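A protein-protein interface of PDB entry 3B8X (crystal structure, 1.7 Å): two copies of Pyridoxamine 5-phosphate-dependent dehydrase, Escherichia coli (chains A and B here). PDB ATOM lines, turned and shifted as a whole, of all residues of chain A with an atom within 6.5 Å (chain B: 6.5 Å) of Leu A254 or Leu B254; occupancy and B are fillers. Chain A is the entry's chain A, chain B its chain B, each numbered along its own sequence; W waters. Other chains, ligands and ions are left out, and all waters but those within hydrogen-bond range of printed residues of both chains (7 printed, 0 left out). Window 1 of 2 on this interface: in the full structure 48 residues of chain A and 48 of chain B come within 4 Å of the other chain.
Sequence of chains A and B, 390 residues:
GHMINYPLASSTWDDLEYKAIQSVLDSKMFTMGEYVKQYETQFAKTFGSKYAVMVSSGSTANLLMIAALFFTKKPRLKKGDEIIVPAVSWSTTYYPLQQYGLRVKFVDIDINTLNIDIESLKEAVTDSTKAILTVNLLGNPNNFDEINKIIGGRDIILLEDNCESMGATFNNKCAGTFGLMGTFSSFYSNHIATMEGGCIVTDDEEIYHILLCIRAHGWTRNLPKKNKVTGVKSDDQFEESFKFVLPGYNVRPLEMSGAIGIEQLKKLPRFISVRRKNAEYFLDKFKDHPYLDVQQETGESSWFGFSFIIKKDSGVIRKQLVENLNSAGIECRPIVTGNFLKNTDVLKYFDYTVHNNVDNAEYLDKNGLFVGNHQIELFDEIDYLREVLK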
ATOM      1  N   PHE A  30      20.565  12.738  -8.373  1.00  0.00           N
ATOM      2  CA  PHE A  30      21.325  12.505  -9.576  1.00  0.00           C
ATOM      3  C   PHE A  30      22.829  12.453  -9.469  1.00  0.00           C
ATOM      4  O   PHE A  30      23.502  11.838 -10.289  1.00  0.00           O
ATOM      5  CB  PHE A  30      20.920  13.531 -10.659  1.00  0.00           C
ATOM      6  CG  PHE A  30      19.435  13.514 -10.953  1.00  0.00           C
ATOM      7  CD1 PHE A  30      18.584  14.455 -10.382  1.00  0.00           C
ATOM      8  CD2 PHE A  30      18.873  12.447 -11.651  1.00  0.00           C
ATOM      9  CE1 PHE A  30      17.196  14.362 -10.548  1.00  0.00           C
ATOM     10  CE2 PHE A  30      17.486  12.368 -11.860  1.00  0.00           C
ATOM     11  CZ  PHE A  30      16.654  13.340 -11.330  1.00  0.00           C
ATOM     12  N   THR A  31      23.325  13.196  -8.497  1.00  0.00           N
ATOM     13  CA  THR A  31      24.756  13.340  -8.273  1.00  0.00           C
ATOM     14  C   THR A  31      25.260  12.009  -7.747  1.00  0.00           C
ATOM     15  O   THR A  31      24.556  11.310  -7.002  1.00  0.00           O
ATOM     16  CB  THR A  31      24.924  14.397  -7.203  1.00  0.00           C
ATOM     17  OG1 THR A  31      24.386  15.607  -7.739  1.00  0.00           O
ATOM     18  CG2 THR A  31      26.343  14.558  -6.814  1.00  0.00           C
ATOM     19  N   MET A  32      26.474  11.662  -8.157  1.00  0.00           N
ATOM     20  CA  MET A  32      27.143  10.449  -7.740  1.00  0.00           C
ATOM     21  C   MET A  32      26.763  10.158  -6.297  1.00  0.00           C
ATOM     22  O   MET A  32      27.017  10.950  -5.420  1.00  0.00           O
ATOM     23  CB  MET A  32      28.657  10.637  -7.843  1.00  0.00           C
ATOM     24  CG  MET A  32      29.517   9.365  -7.570  1.00  0.00           C
ATOM     25  SD  MET A  32      31.224   9.856  -7.325  1.00  0.00           S
ATOM     26  CE  MET A  32      31.261  10.549  -5.664  1.00  0.00           C
ATOM     27  N   GLY A  33      26.205   8.988  -6.043  1.00  0.00           N
ATOM     28  CA  GLY A  33      25.771   8.641  -4.699  1.00  0.00           C
ATOM     29  C   GLY A  33      25.596   7.163  -4.435  1.00  0.00           C
ATOM     30  O   GLY A  33      26.501   6.357  -4.642  1.00  0.00           O
ATOM     31  N   VAL A  36      25.973   4.473  -7.391  1.00  0.00           N
ATOM     32  CA  VAL A  36      27.374   4.332  -7.731  1.00  0.00           C
ATOM     33  C   VAL A  36      28.109   3.540  -6.660  1.00  0.00           C
ATOM     34  O   VAL A  36      28.868   2.634  -6.984  1.00  0.00           O
ATOM     35  CB  VAL A  36      28.077   5.684  -7.885  1.00  0.00           C
ATOM     36  CG1 VAL A  36      29.606   5.475  -8.108  1.00  0.00           C
ATOM     37  CG2 VAL A  36      27.449   6.488  -9.015  1.00  0.00           C
ATOM     38  N   MET A  54      34.221   4.027  -9.602  1.00  0.00           N
ATOM     39  CA  MET A  54      33.608   4.358 -10.887  1.00  0.00           C
ATOM     40  C   MET A  54      33.923   5.782 -11.277  1.00  0.00           C
ATOM     41  O   MET A  54      33.900   6.657 -10.418  1.00  0.00           O
ATOM     42  CB  MET A  54      32.107   4.124 -10.876  1.00  0.00           C
ATOM     43  CG  MET A  54      31.438   4.274 -12.254  1.00  0.00           C
ATOM     44  SD  MET A  54      29.640   4.199 -12.099  1.00  0.00           S
ATOM     45  CE  MET A  54      29.241   3.776 -13.828  1.00  0.00           C
ATOM     46  N   VAL A  55      34.193   6.021 -12.565  1.00  0.00           N
ATOM     47  CA  VAL A  55      34.527   7.344 -13.084  1.00  0.00           C
ATOM     48  C   VAL A  55      33.712   7.608 -14.364  1.00  0.00           C
ATOM     49  O   VAL A  55      32.940   6.762 -14.806  1.00  0.00           O
ATOM     50  CB  VAL A  55      36.036   7.540 -13.296  1.00  0.00           C
ATOM     51  CG1 VAL A  55      36.797   7.675 -11.972  1.00  0.00           C
ATOM     52  CG2 VAL A  55      36.635   6.377 -14.149  1.00  0.00           C
ATOM     53  N   SER A  56      33.855   8.805 -14.922  1.00  0.00           N
ATOM     54  CA  SER A  56      33.089   9.255 -16.093  1.00  0.00           C
ATOM     55  C   SER A  56      33.309   8.464 -17.378  1.00  0.00           C
ATOM     56  O   SER A  56      32.437   8.394 -18.259  1.00  0.00           O
ATOM     57  CB  SER A  56      33.316  10.749 -16.370  1.00  0.00           C
ATOM     58  OG  SER A  56      34.691  10.982 -16.676  1.00  0.00           O
ATOM     59  N   THR A 194      26.953   1.986 -19.822  1.00  0.00           N
ATOM     60  CA  THR A 194      26.272   2.845 -18.841  1.00  0.00           C
ATOM     61  C   THR A 194      26.146   4.260 -19.418  1.00  0.00           C
ATOM     62  O   THR A 194      26.143   5.265 -18.681  1.00  0.00           O
ATOM     63  CB  THR A 194      27.073   2.928 -17.528  1.00  0.00           C
ATOM     64  OG1 THR A 194      28.417   3.397 -17.765  1.00  0.00           O
ATOM     65  CG2 THR A 194      27.135   1.591 -16.853  1.00  0.00           C
ATOM     66  N   MET A 195      26.031   4.300 -20.747  1.00  0.00           N
ATOM     67  CA  MET A 195      26.008   5.524 -21.562  1.00  0.00           C
ATOM     68  C   MET A 195      27.489   5.890 -21.737  1.00  0.00           C
ATOM     69  O   MET A 195      28.064   5.724 -22.822  1.00  0.00           O
ATOM     70  CB  MET A 195      25.139   6.633 -20.960  1.00  0.00           C
ATOM     71  CG  MET A 195      23.664   6.151 -20.713  1.00  0.00           C
ATOM     72  SD  MET A 195      22.498   7.453 -20.232  1.00  0.00           S
ATOM     73  CE  MET A 195      22.834   7.819 -18.525  1.00  0.00           C
ATOM     74  N   GLU A 196      28.117   6.320 -20.645  1.00  0.00           N
ATOM     75  CA  GLU A 196      29.572   6.489 -20.632  1.00  0.00           C
ATOM     76  C   GLU A 196      29.894   5.965 -19.258  1.00  0.00           C
ATOM     77  O   GLU A 196      29.005   5.887 -18.399  1.00  0.00           O
ATOM     78  CB  GLU A 196      30.054   7.934 -20.745  1.00  0.00           C
ATOM     79  CG  GLU A 196      29.730   8.489 -22.108  1.00  0.00           C
ATOM     80  CD  GLU A 196      30.934   8.867 -22.912  1.00  0.00           C
ATOM     81  OE1 GLU A 196      32.014   8.270 -22.719  1.00  0.00           O
ATOM     82  OE2 GLU A 196      30.779   9.770 -23.750  1.00  0.00           O
ATOM     83  N   ARG A 252      33.495  12.497 -11.708  1.00  0.00           N
ATOM     84  CA  ARG A 252      32.448  11.686 -11.094  1.00  0.00           C
ATOM     85  C   ARG A 252      31.527  11.165 -12.151  1.00  0.00           C
ATOM     86  O   ARG A 252      31.224  11.851 -13.137  1.00  0.00           O
ATOM     87  CB  ARG A 252      31.646  12.537 -10.113  1.00  0.00           C
ATOM     88  CG  ARG A 252      32.494  12.929  -8.962  1.00  0.00           C
ATOM     89  CD  ARG A 252      31.682  13.659  -7.878  1.00  0.00           C
ATOM     90  NE  ARG A 252      30.814  14.697  -8.401  1.00  0.00           N
ATOM     91  CZ  ARG A 252      30.291  15.642  -7.591  1.00  0.00           C
ATOM     92  NH1 ARG A 252      30.543  15.631  -6.281  1.00  0.00           N
ATOM     93  NH2 ARG A 252      29.485  16.591  -8.064  1.00  0.00           N
ATOM     94  N   PRO A 253      31.058   9.948 -11.929  1.00  0.00           N
ATOM     95  CA  PRO A 253      30.110   9.358 -12.870  1.00  0.00           C
ATOM     96  C   PRO A 253      28.763   9.863 -12.332  1.00  0.00           C
ATOM     97  O   PRO A 253      28.741  10.411 -11.239  1.00  0.00           O
ATOM     98  CB  PRO A 253      30.301   7.858 -12.667  1.00  0.00           C
ATOM     99  CG  PRO A 253      30.611   7.774 -11.229  1.00  0.00           C
ATOM    100  CD  PRO A 253      31.586   8.959 -10.976  1.00  0.00           C
ATOM    101  N   LEU A 254      27.672   9.690 -13.090  1.00  0.00           N
ATOM    102  CA  LEU A 254      26.295  10.083 -12.683  1.00  0.00           C
ATOM    103  C   LEU A 254      25.616   8.884 -12.010  1.00  0.00           C
ATOM    104  O   LEU A 254      26.014   7.742 -12.323  1.00  0.00           O
ATOM    105  CB  LEU A 254      25.502  10.447 -13.943  1.00  0.00           C
ATOM    106  CG  LEU A 254      25.906  11.702 -14.706  1.00  0.00           C
ATOM    107  CD1 LEU A 254      24.811  11.953 -15.751  1.00  0.00           C
ATOM    108  CD2 LEU A 254      26.000  12.884 -13.737  1.00  0.00           C
ATOM    109  N   GLU A 255      24.650   9.126 -11.101  1.00  0.00           N
ATOM    110  CA  GLU A 255      23.885   8.074 -10.421  1.00  0.00           C
ATOM    111  C   GLU A 255      23.187   7.176 -11.451  1.00  0.00           C
ATOM    112  O   GLU A 255      23.119   5.967 -11.268  1.00  0.00           O
ATOM    113  CB  GLU A 255      22.772   8.669  -9.536  1.00  0.00           C
ATOM    114  CG  GLU A 255      23.051   8.833  -8.046  1.00  0.00           C
ATOM    115  CD  GLU A 255      23.496   7.568  -7.323  1.00  0.00           C
ATOM    116  OE1 GLU A 255      24.666   7.156  -7.466  1.00  0.00           O
ATOM    117  OE2 GLU A 255      22.681   6.971  -6.594  1.00  0.00           O
ATOM    118  N   MET A 256      22.704   7.741 -12.566  1.00  0.00           N
ATOM    119  CA  MET A 256      22.084   6.888 -13.592  1.00  0.00           C
ATOM    120  C   MET A 256      23.041   5.811 -14.078  1.00  0.00           C
ATOM    121  O   MET A 256      22.648   4.689 -14.174  1.00  0.00           O
ATOM    122  CB  MET A 256      21.615   7.684 -14.816  1.00  0.00           C
ATOM    123  CG  MET A 256      20.308   8.433 -14.527  1.00  0.00           C
ATOM    124  SD  MET A 256      20.001   9.424 -15.952  1.00  0.00           S
ATOM    125  CE  MET A 256      18.396  10.228 -15.561  1.00  0.00           C
ATOM    126  N   SER A 257      24.266   6.179 -14.432  1.00  0.00           N
ATOM    127  CA  SER A 257      25.276   5.220 -14.915  1.00  0.00           C
ATOM    128  C   SER A 257      25.542   4.131 -13.878  1.00  0.00           C
ATOM    129  O   SER A 257      25.714   2.957 -14.204  1.00  0.00           O
ATOM    130  CB  SER A 257      26.551   5.983 -15.254  1.00  0.00           C
ATOM    131  OG  SER A 257      26.260   6.802 -16.380  1.00  0.00           O
ATOM    132  N   GLY A 258      25.590   4.523 -12.615  1.00  0.00           N
ATOM    133  CA  GLY A 258      25.781   3.524 -11.556  1.00  0.00           C
ATOM    134  C   GLY A 258      24.584   2.544 -11.526  1.00  0.00           C
ATOM    135  O   GLY A 258      24.764   1.321 -11.455  1.00  0.00           O
ATOM    136  N   ALA A 259      23.369   3.110 -11.537  1.00  0.00           N
ATOM    137  CA  ALA A 259      22.133   2.323 -11.488  1.00  0.00           C
ATOM    138  C   ALA A 259      22.083   1.392 -12.700  1.00  0.00           C
ATOM    139  O   ALA A 259      21.820   0.206 -12.564  1.00  0.00           O
ATOM    140  CB  ALA A 259      20.944   3.247 -11.447  1.00  0.00           C
ATOM    141  N   PHE B  30      22.335   7.690 -26.539  1.00  0.00           N
ATOM    142  CA  PHE B  30      22.783   8.276 -25.284  1.00  0.00           C
ATOM    143  C   PHE B  30      24.103   9.027 -25.329  1.00  0.00           C
ATOM    144  O   PHE B  30      24.383   9.918 -24.512  1.00  0.00           O
ATOM    145  CB  PHE B  30      22.819   7.155 -24.230  1.00  0.00           C
ATOM    146  CG  PHE B  30      21.485   6.473 -24.061  1.00  0.00           C
ATOM    147  CD1 PHE B  30      21.241   5.243 -24.646  1.00  0.00           C
ATOM    148  CD2 PHE B  30      20.418   7.152 -23.484  1.00  0.00           C
ATOM    149  CE1 PHE B  30      19.973   4.660 -24.575  1.00  0.00           C
ATOM    150  CE2 PHE B  30      19.143   6.568 -23.403  1.00  0.00           C
ATOM    151  CZ  PHE B  30      18.924   5.331 -23.958  1.00  0.00           C
ATOM    152  N   THR B  31      24.922   8.667 -26.295  1.00  0.00           N
ATOM    153  CA  THR B  31      26.224   9.278 -26.392  1.00  0.00           C
ATOM    154  C   THR B  31      26.056  10.632 -26.982  1.00  0.00           C
ATOM    155  O   THR B  31      25.216  10.815 -27.850  1.00  0.00           O
ATOM    156  CB  THR B  31      27.127   8.485 -27.339  1.00  0.00           C
ATOM    157  OG1 THR B  31      27.336   7.193 -26.762  1.00  0.00           O
ATOM    158  CG2 THR B  31      28.460   9.199 -27.499  1.00  0.00           C
ATOM    159  N   MET B  32      26.932  11.541 -26.565  1.00  0.00           N
ATOM    160  CA  MET B  32      26.997  12.899 -27.087  1.00  0.00           C
ATOM    161  C   MET B  32      26.597  12.934 -28.570  1.00  0.00           C
ATOM    162  O   MET B  32      27.239  12.297 -29.431  1.00  0.00           O
ATOM    163  CB  MET B  32      28.440  13.404 -26.928  1.00  0.00           C
ATOM    164  CG  MET B  32      28.552  14.891 -27.148  1.00  0.00           C
ATOM    165  SD  MET B  32      30.306  15.343 -27.230  1.00  0.00           S
ATOM    166  CE  MET B  32      30.903  14.610 -28.774  1.00  0.00           C
ATOM    167  N   GLY B  33      25.557  13.713 -28.868  1.00  0.00           N
ATOM    168  CA  GLY B  33      25.088  13.856 -30.244  1.00  0.00           C
ATOM    169  C   GLY B  33      24.359  15.191 -30.490  1.00  0.00           C
ATOM    170  O   GLY B  33      24.840  16.306 -30.198  1.00  0.00           O
ATOM    171  N   VAL B  36      23.218  17.646 -27.538  1.00  0.00           N
ATOM    172  CA  VAL B  36      24.354  18.411 -27.058  1.00  0.00           C
ATOM    173  C   VAL B  36      24.674  19.519 -28.071  1.00  0.00           C
ATOM    174  O   VAL B  36      24.948  20.654 -27.713  1.00  0.00           O
ATOM    175  CB  VAL B  36      25.624  17.519 -26.895  1.00  0.00           C
ATOM    176  CG1 VAL B  36      26.883  18.406 -26.736  1.00  0.00           C
ATOM    177  CG2 VAL B  36      25.426  16.559 -25.724  1.00  0.00           C
ATOM    178  N   MET B  54      30.185  21.946 -24.859  1.00  0.00           N
ATOM    179  CA  MET B  54      29.731  21.304 -23.622  1.00  0.00           C
ATOM    180  C   MET B  54      30.613  20.134 -23.208  1.00  0.00           C
ATOM    181  O   MET B  54      31.041  19.361 -24.050  1.00  0.00           O
ATOM    182  CB  MET B  54      28.348  20.748 -23.789  1.00  0.00           C
ATOM    183  CG  MET B  54      27.720  20.329 -22.423  1.00  0.00           C
ATOM    184  SD  MET B  54      26.107  19.525 -22.689  1.00  0.00           S
ATOM    185  CE  MET B  54      25.347  19.516 -21.047  1.00  0.00           C
ATOM    186  N   VAL B  55      30.894  20.030 -21.923  1.00  0.00           N
ATOM    187  CA  VAL B  55      31.785  18.993 -21.420  1.00  0.00           C
ATOM    188  C   VAL B  55      31.200  18.394 -20.167  1.00  0.00           C
ATOM    189  O   VAL B  55      30.152  18.801 -19.677  1.00  0.00           O
ATOM    190  CB  VAL B  55      33.238  19.495 -21.142  1.00  0.00           C
ATOM    191  CG1 VAL B  55      33.954  19.779 -22.477  1.00  0.00           C
ATOM    192  CG2 VAL B  55      33.223  20.730 -20.295  1.00  0.00           C
ATOM    193  N   SER B  56      31.857  17.371 -19.677  1.00  0.00           N
ATOM    194  CA  SER B  56      31.325  16.661 -18.539  1.00  0.00           C
ATOM    195  C   SER B  56      31.082  17.458 -17.259  1.00  0.00           C
ATOM    196  O   SER B  56      30.233  17.054 -16.491  1.00  0.00           O
ATOM    197  CB  SER B  56      32.159  15.393 -18.314  1.00  0.00           C
ATOM    198  OG  SER B  56      33.468  15.712 -17.815  1.00  0.00           O
ATOM    199  N   THR B 194      22.187  20.006 -15.036  1.00  0.00           N
ATOM    200  CA  THR B 194      22.022  18.938 -16.010  1.00  0.00           C
ATOM    201  C   THR B 194      22.632  17.670 -15.398  1.00  0.00           C
ATOM    202  O   THR B 194      23.245  16.860 -16.083  1.00  0.00           O
ATOM    203  CB  THR B 194      22.798  19.306 -17.294  1.00  0.00           C
ATOM    204  OG1 THR B 194      24.188  19.495 -16.973  1.00  0.00           O
ATOM    205  CG2 THR B 194      22.282  20.597 -17.840  1.00  0.00           C
ATOM    206  N   MET B 195      22.460  17.515 -14.095  1.00  0.00           N
ATOM    207  CA  MET B 195      23.057  16.412 -13.328  1.00  0.00           C
ATOM    208  C   MET B 195      24.533  16.774 -13.058  1.00  0.00           C
ATOM    209  O   MET B 195      24.879  17.058 -11.922  1.00  0.00           O
ATOM    210  CB  MET B 195      22.837  15.042 -14.010  1.00  0.00           C
ATOM    211  CG  MET B 195      21.365  14.811 -14.281  1.00  0.00           C
ATOM    212  SD  MET B 195      20.983  13.112 -14.767  1.00  0.00           S
ATOM    213  CE  MET B 195      21.434  13.166 -16.409  1.00  0.00           C
ATOM    214  N   GLU B 196      25.390  16.775 -14.083  1.00  0.00           N
ATOM    215  CA  GLU B 196      26.742  17.298 -13.991  1.00  0.00           C
ATOM    216  C   GLU B 196      26.831  17.958 -15.372  1.00  0.00           C
ATOM    217  O   GLU B 196      26.068  17.587 -16.281  1.00  0.00           O
ATOM    218  CB  GLU B 196      27.800  16.181 -13.881  1.00  0.00           C
ATOM    219  CG  GLU B 196      27.835  15.468 -12.534  1.00  0.00           C
ATOM    220  CD  GLU B 196      28.859  15.987 -11.552  1.00  0.00           C
ATOM    221  OE1 GLU B 196      29.514  17.038 -11.757  1.00  0.00           O
ATOM    222  OE2 GLU B 196      28.986  15.333 -10.520  1.00  0.00           O
ATOM    223  N   ARG B 252      33.418  14.014 -22.624  1.00  0.00           N
ATOM    224  CA  ARG B 252      32.172  14.281 -23.283  1.00  0.00           C
ATOM    225  C   ARG B 252      31.034  14.284 -22.248  1.00  0.00           C
ATOM    226  O   ARG B 252      31.123  13.586 -21.235  1.00  0.00           O
ATOM    227  CB  ARG B 252      31.920  13.153 -24.300  1.00  0.00           C
ATOM    228  CG  ARG B 252      32.840  13.141 -25.497  1.00  0.00           C
ATOM    229  CD  ARG B 252      32.368  12.064 -26.444  1.00  0.00           C
ATOM    230  NE  ARG B 252      32.393  10.706 -25.902  1.00  0.00           N
ATOM    231  CZ  ARG B 252      32.652   9.624 -26.632  1.00  0.00           C
ATOM    232  NH1 ARG B 252      32.886   9.745 -27.938  1.00  0.00           N
ATOM    233  NH2 ARG B 252      32.667   8.419 -26.063  1.00  0.00           N
ATOM    234  N   PRO B 253      29.985  15.082 -22.477  1.00  0.00           N
ATOM    235  CA  PRO B 253      28.849  15.071 -21.564  1.00  0.00           C
ATOM    236  C   PRO B 253      27.927  14.014 -22.138  1.00  0.00           C
ATOM    237  O   PRO B 253      28.111  13.577 -23.272  1.00  0.00           O
ATOM    238  CB  PRO B 253      28.156  16.443 -21.809  1.00  0.00           C
ATOM    239  CG  PRO B 253      28.623  16.904 -23.199  1.00  0.00           C
ATOM    240  CD  PRO B 253      29.816  16.048 -23.588  1.00  0.00           C
ATOM    241  N   LEU B 254      26.861  13.694 -21.410  1.00  0.00           N
ATOM    242  CA  LEU B 254      25.885  12.710 -21.892  1.00  0.00           C
ATOM    243  C   LEU B 254      24.826  13.390 -22.744  1.00  0.00           C
ATOM    244  O   LEU B 254      24.530  14.568 -22.544  1.00  0.00           O
ATOM    245  CB  LEU B 254      25.217  12.021 -20.716  1.00  0.00           C
ATOM    246  CG  LEU B 254      26.194  11.094 -19.978  1.00  0.00           C
ATOM    247  CD1 LEU B 254      25.530  10.497 -18.771  1.00  0.00           C
ATOM    248  CD2 LEU B 254      26.720  10.043 -20.918  1.00  0.00           C
ATOM    249  N   GLU B 255      24.202  12.646 -23.659  1.00  0.00           N
ATOM    250  CA  GLU B 255      23.134  13.253 -24.452  1.00  0.00           C
ATOM    251  C   GLU B 255      21.967  13.791 -23.577  1.00  0.00           C
ATOM    252  O   GLU B 255      21.305  14.795 -23.885  1.00  0.00           O
ATOM    253  CB  GLU B 255      22.635  12.245 -25.475  1.00  0.00           C
ATOM    254  CG  GLU B 255      21.689  12.869 -26.405  1.00  0.00           C
ATOM    255  CD  GLU B 255      22.317  13.684 -27.539  1.00  0.00           C
ATOM    256  OE1 GLU B 255      23.347  14.403 -27.391  1.00  0.00           O
ATOM    257  OE2 GLU B 255      21.712  13.648 -28.623  1.00  0.00           O
ATOM    258  N   MET B 256      21.718  13.116 -22.453  1.00  0.00           N
ATOM    259  CA  MET B 256      20.675  13.533 -21.549  1.00  0.00           C
ATOM    260  C   MET B 256      20.985  14.906 -20.983  1.00  0.00           C
ATOM    261  O   MET B 256      20.070  15.721 -20.797  1.00  0.00           O
ATOM    262  CB  MET B 256      20.562  12.542 -20.392  1.00  0.00           C
ATOM    263  CG  MET B 256      19.673  11.362 -20.721  1.00  0.00           C
ATOM    264  SD  MET B 256      19.832  10.370 -19.246  1.00  0.00           S
ATOM    265  CE  MET B 256      18.987   8.855 -19.641  1.00  0.00           C
ATOM    266  N   SER B 257      22.255  15.141 -20.664  1.00  0.00           N
ATOM    267  CA  SER B 257      22.617  16.426 -20.090  1.00  0.00           C
ATOM    268  C   SER B 257      22.328  17.573 -21.056  1.00  0.00           C
ATOM    269  O   SER B 257      21.921  18.650 -20.651  1.00  0.00           O
ATOM    270  CB  SER B 257      24.052  16.460 -19.631  1.00  0.00           C
ATOM    271  OG  SER B 257      24.171  15.693 -18.446  1.00  0.00           O
ATOM    272  N   GLY B 258      22.585  17.345 -22.331  1.00  0.00           N
ATOM    273  CA  GLY B 258      22.346  18.358 -23.352  1.00  0.00           C
ATOM    274  C   GLY B 258      20.825  18.581 -23.489  1.00  0.00           C
ATOM    275  O   GLY B 258      20.371  19.705 -23.577  1.00  0.00           O
ATOM    276  N   ALA B 259      20.025  17.529 -23.404  1.00  0.00           N
ATOM    277  CA  ALA B 259      18.584  17.695 -23.533  1.00  0.00           C
ATOM    278  C   ALA B 259      18.026  18.499 -22.387  1.00  0.00           C
ATOM    279  O   ALA B 259      17.236  19.420 -22.590  1.00  0.00           O
ATOM    280  CB  ALA B 259      17.854  16.360 -23.680  1.00  0.00           C
HETATM  281  O   HOH W   1      28.539  11.010 -24.357  1.00  0.00           O
HETATM  282  O   HOH W   2      27.805  13.065 -10.355  1.00  0.00           O
HETATM  283  O   HOH W   3      26.148   5.672 -24.996  1.00  0.00           O
HETATM  284  O   HOH W   4      32.548  11.152 -20.878  1.00  0.00           O
HETATM  285  O   HOH W   5      22.166  10.744 -12.504  1.00  0.00           O
HETATM  286  O   HOH W   6      23.016  16.371  -9.976  1.00  0.00           O
HETATM  287  O   HOH W   7      22.566  10.104 -22.400  1.00  0.00           O
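The guanidinium group (NH2) of Arg A252 is in salt-bridge range of the side-chain carboxylate (OE2) of Glu B196, at 2.8 Å. NE of Arg B252 lies within salt-bridge range of OE2 of Glu A196. The side-chain sulfur (SD) of Met B256 lies close to the side-chain sulfur (SD) of Met A256 (3.4 Å).
The backbone NH of Glu B255 is in hydrogen-bond range of the backbone carbonyl oxygen of Phe B30, 2.9 Å away. The side-chain hydroxyl (OG) of Ser B257 is in hydrogen-bond range of the backbone carbonyl oxygen (O) of Glu B196, 3.4 Å away. OG1 of Thr A194 sits at hydrogen-bond distance from O of Glu A196 (2.6 Å). The backbone carbonyl oxygen of Phe A30 is in hydrogen-bond range of the backbone NH of Glu A255 (3.1 Å). O of Glu B196 lies within hydrogen-bond range of OG1 of Thr B194 (2.8 Å).
Among the printed residues, pairs that only touch across the chains: Leu A254 with Glu B196 (3.4 Å), Leu A254 with Leu B254 (3.4 Å), Glu A196 with Leu B254 (3.6 Å), Leu A254 with Met B195 (3.6 Å), Met A195 with Phe B30 (3.8 Å), Met A195 with Leu B254 (3.8 Å), Phe A30 with Met B195 (3.8 Å), Met A195 with Met B256 (3.8 Å) and Met A256 with Met B195 (3.95 Å).
Of chain B, only Met B195, Glu B196 and Leu B254 come within 4 Å of Leu A254. Of chain A, only Met A195 (3.8 Å), Glu A196 (3.6 Å) and Leu A254 (3.4 Å) come within 4 Å of Leu B254. Of the printed residues of chain A, Phe B30 touches Met A195. Of the printed residues of chain B, Phe A30 touches Met B195 (3.8 Å). Of the printed residues of chain B, Arg A252 touches Glu B196 (2.8 Å). Of the printed residues of chain B, Met A256 touches Met B195 and Met B256. The nearest residue of chain B that does not touch Leu A254 is Ser B257 (4.7 Å). The nearest residue of chain A that does not touch Leu B254 is Ser A257 (4.5 Å). The nearest printed residue of chain A that does not touch Glu B196 is Thr A31 (4.6 Å).
Hydrophobic or aromatic side chains of chain A within 4 Å of the printed part of chain B: Phe A30, Met A195, Leu A254 and Met A256. Of the 19 printed residues of chain B, 6 touch a printed residue of chain A. Hydrophobic or aromatic side chains of chain B within 4 Å of the printed part of chain A: Phe B30, Met B195, Leu B254 and Met B256. Among the printed residues, Asp or Glu carboxylates within 4 Å of a Lys or Arg side-chain nitrogen of the other chain: Glu A196 with Arg B252 and Arg A252 with Glu B196.
Met A195 touches Leu B254, and with the chains exchanged Leu A254 touches Met B195. Met A195 touches Met B256, and with the chains exchanged Met A256 touches Met B195. Glu A196 touches Leu B254, and with the chains exchanged Leu A254 touches Glu B196. Leu B254 touches its own counterpart, Leu A254. 19 positions are printed for both chains.
Water W2 lies within hydrogen-bond range of OE2 of Glu B196 (2.6 Å), N of Met A32 (2.9 Å) and O of Pro A253 (2.9 Å). Water W1 lies within hydrogen-bond range of OE2 of Glu A196 (2.6 Å), N of Met B32 (2.8 Å) and O of Pro B253 (2.8 Å). Water W6 bridges OG1 of Thr A31 (2.7 Å) and O of Met B195 (2.8 Å). Water W7 lies within hydrogen-bond range of the backbone carbonyl oxygen (O) of Phe B30 (2.8 Å), the backbone NH (N) of Met B256 (3.1 Å), the backbone NH (N) of Glu B255 (3.3 Å) and the side-chain sulfur (SD) of Met A195 (3.4 Å). Water W5 lies within hydrogen-bond range of the backbone carbonyl oxygen (O) of Phe A30, the backbone NH (N) of Met A256, the backbone NH (N) of Glu A255 and the side-chain sulfur (SD) of Met B195. Water W4 bridges the backbone carbonyl oxygen of Arg B252 (2.8 Å) and the side-chain carboxylate of Glu A196 (3.5 Å).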
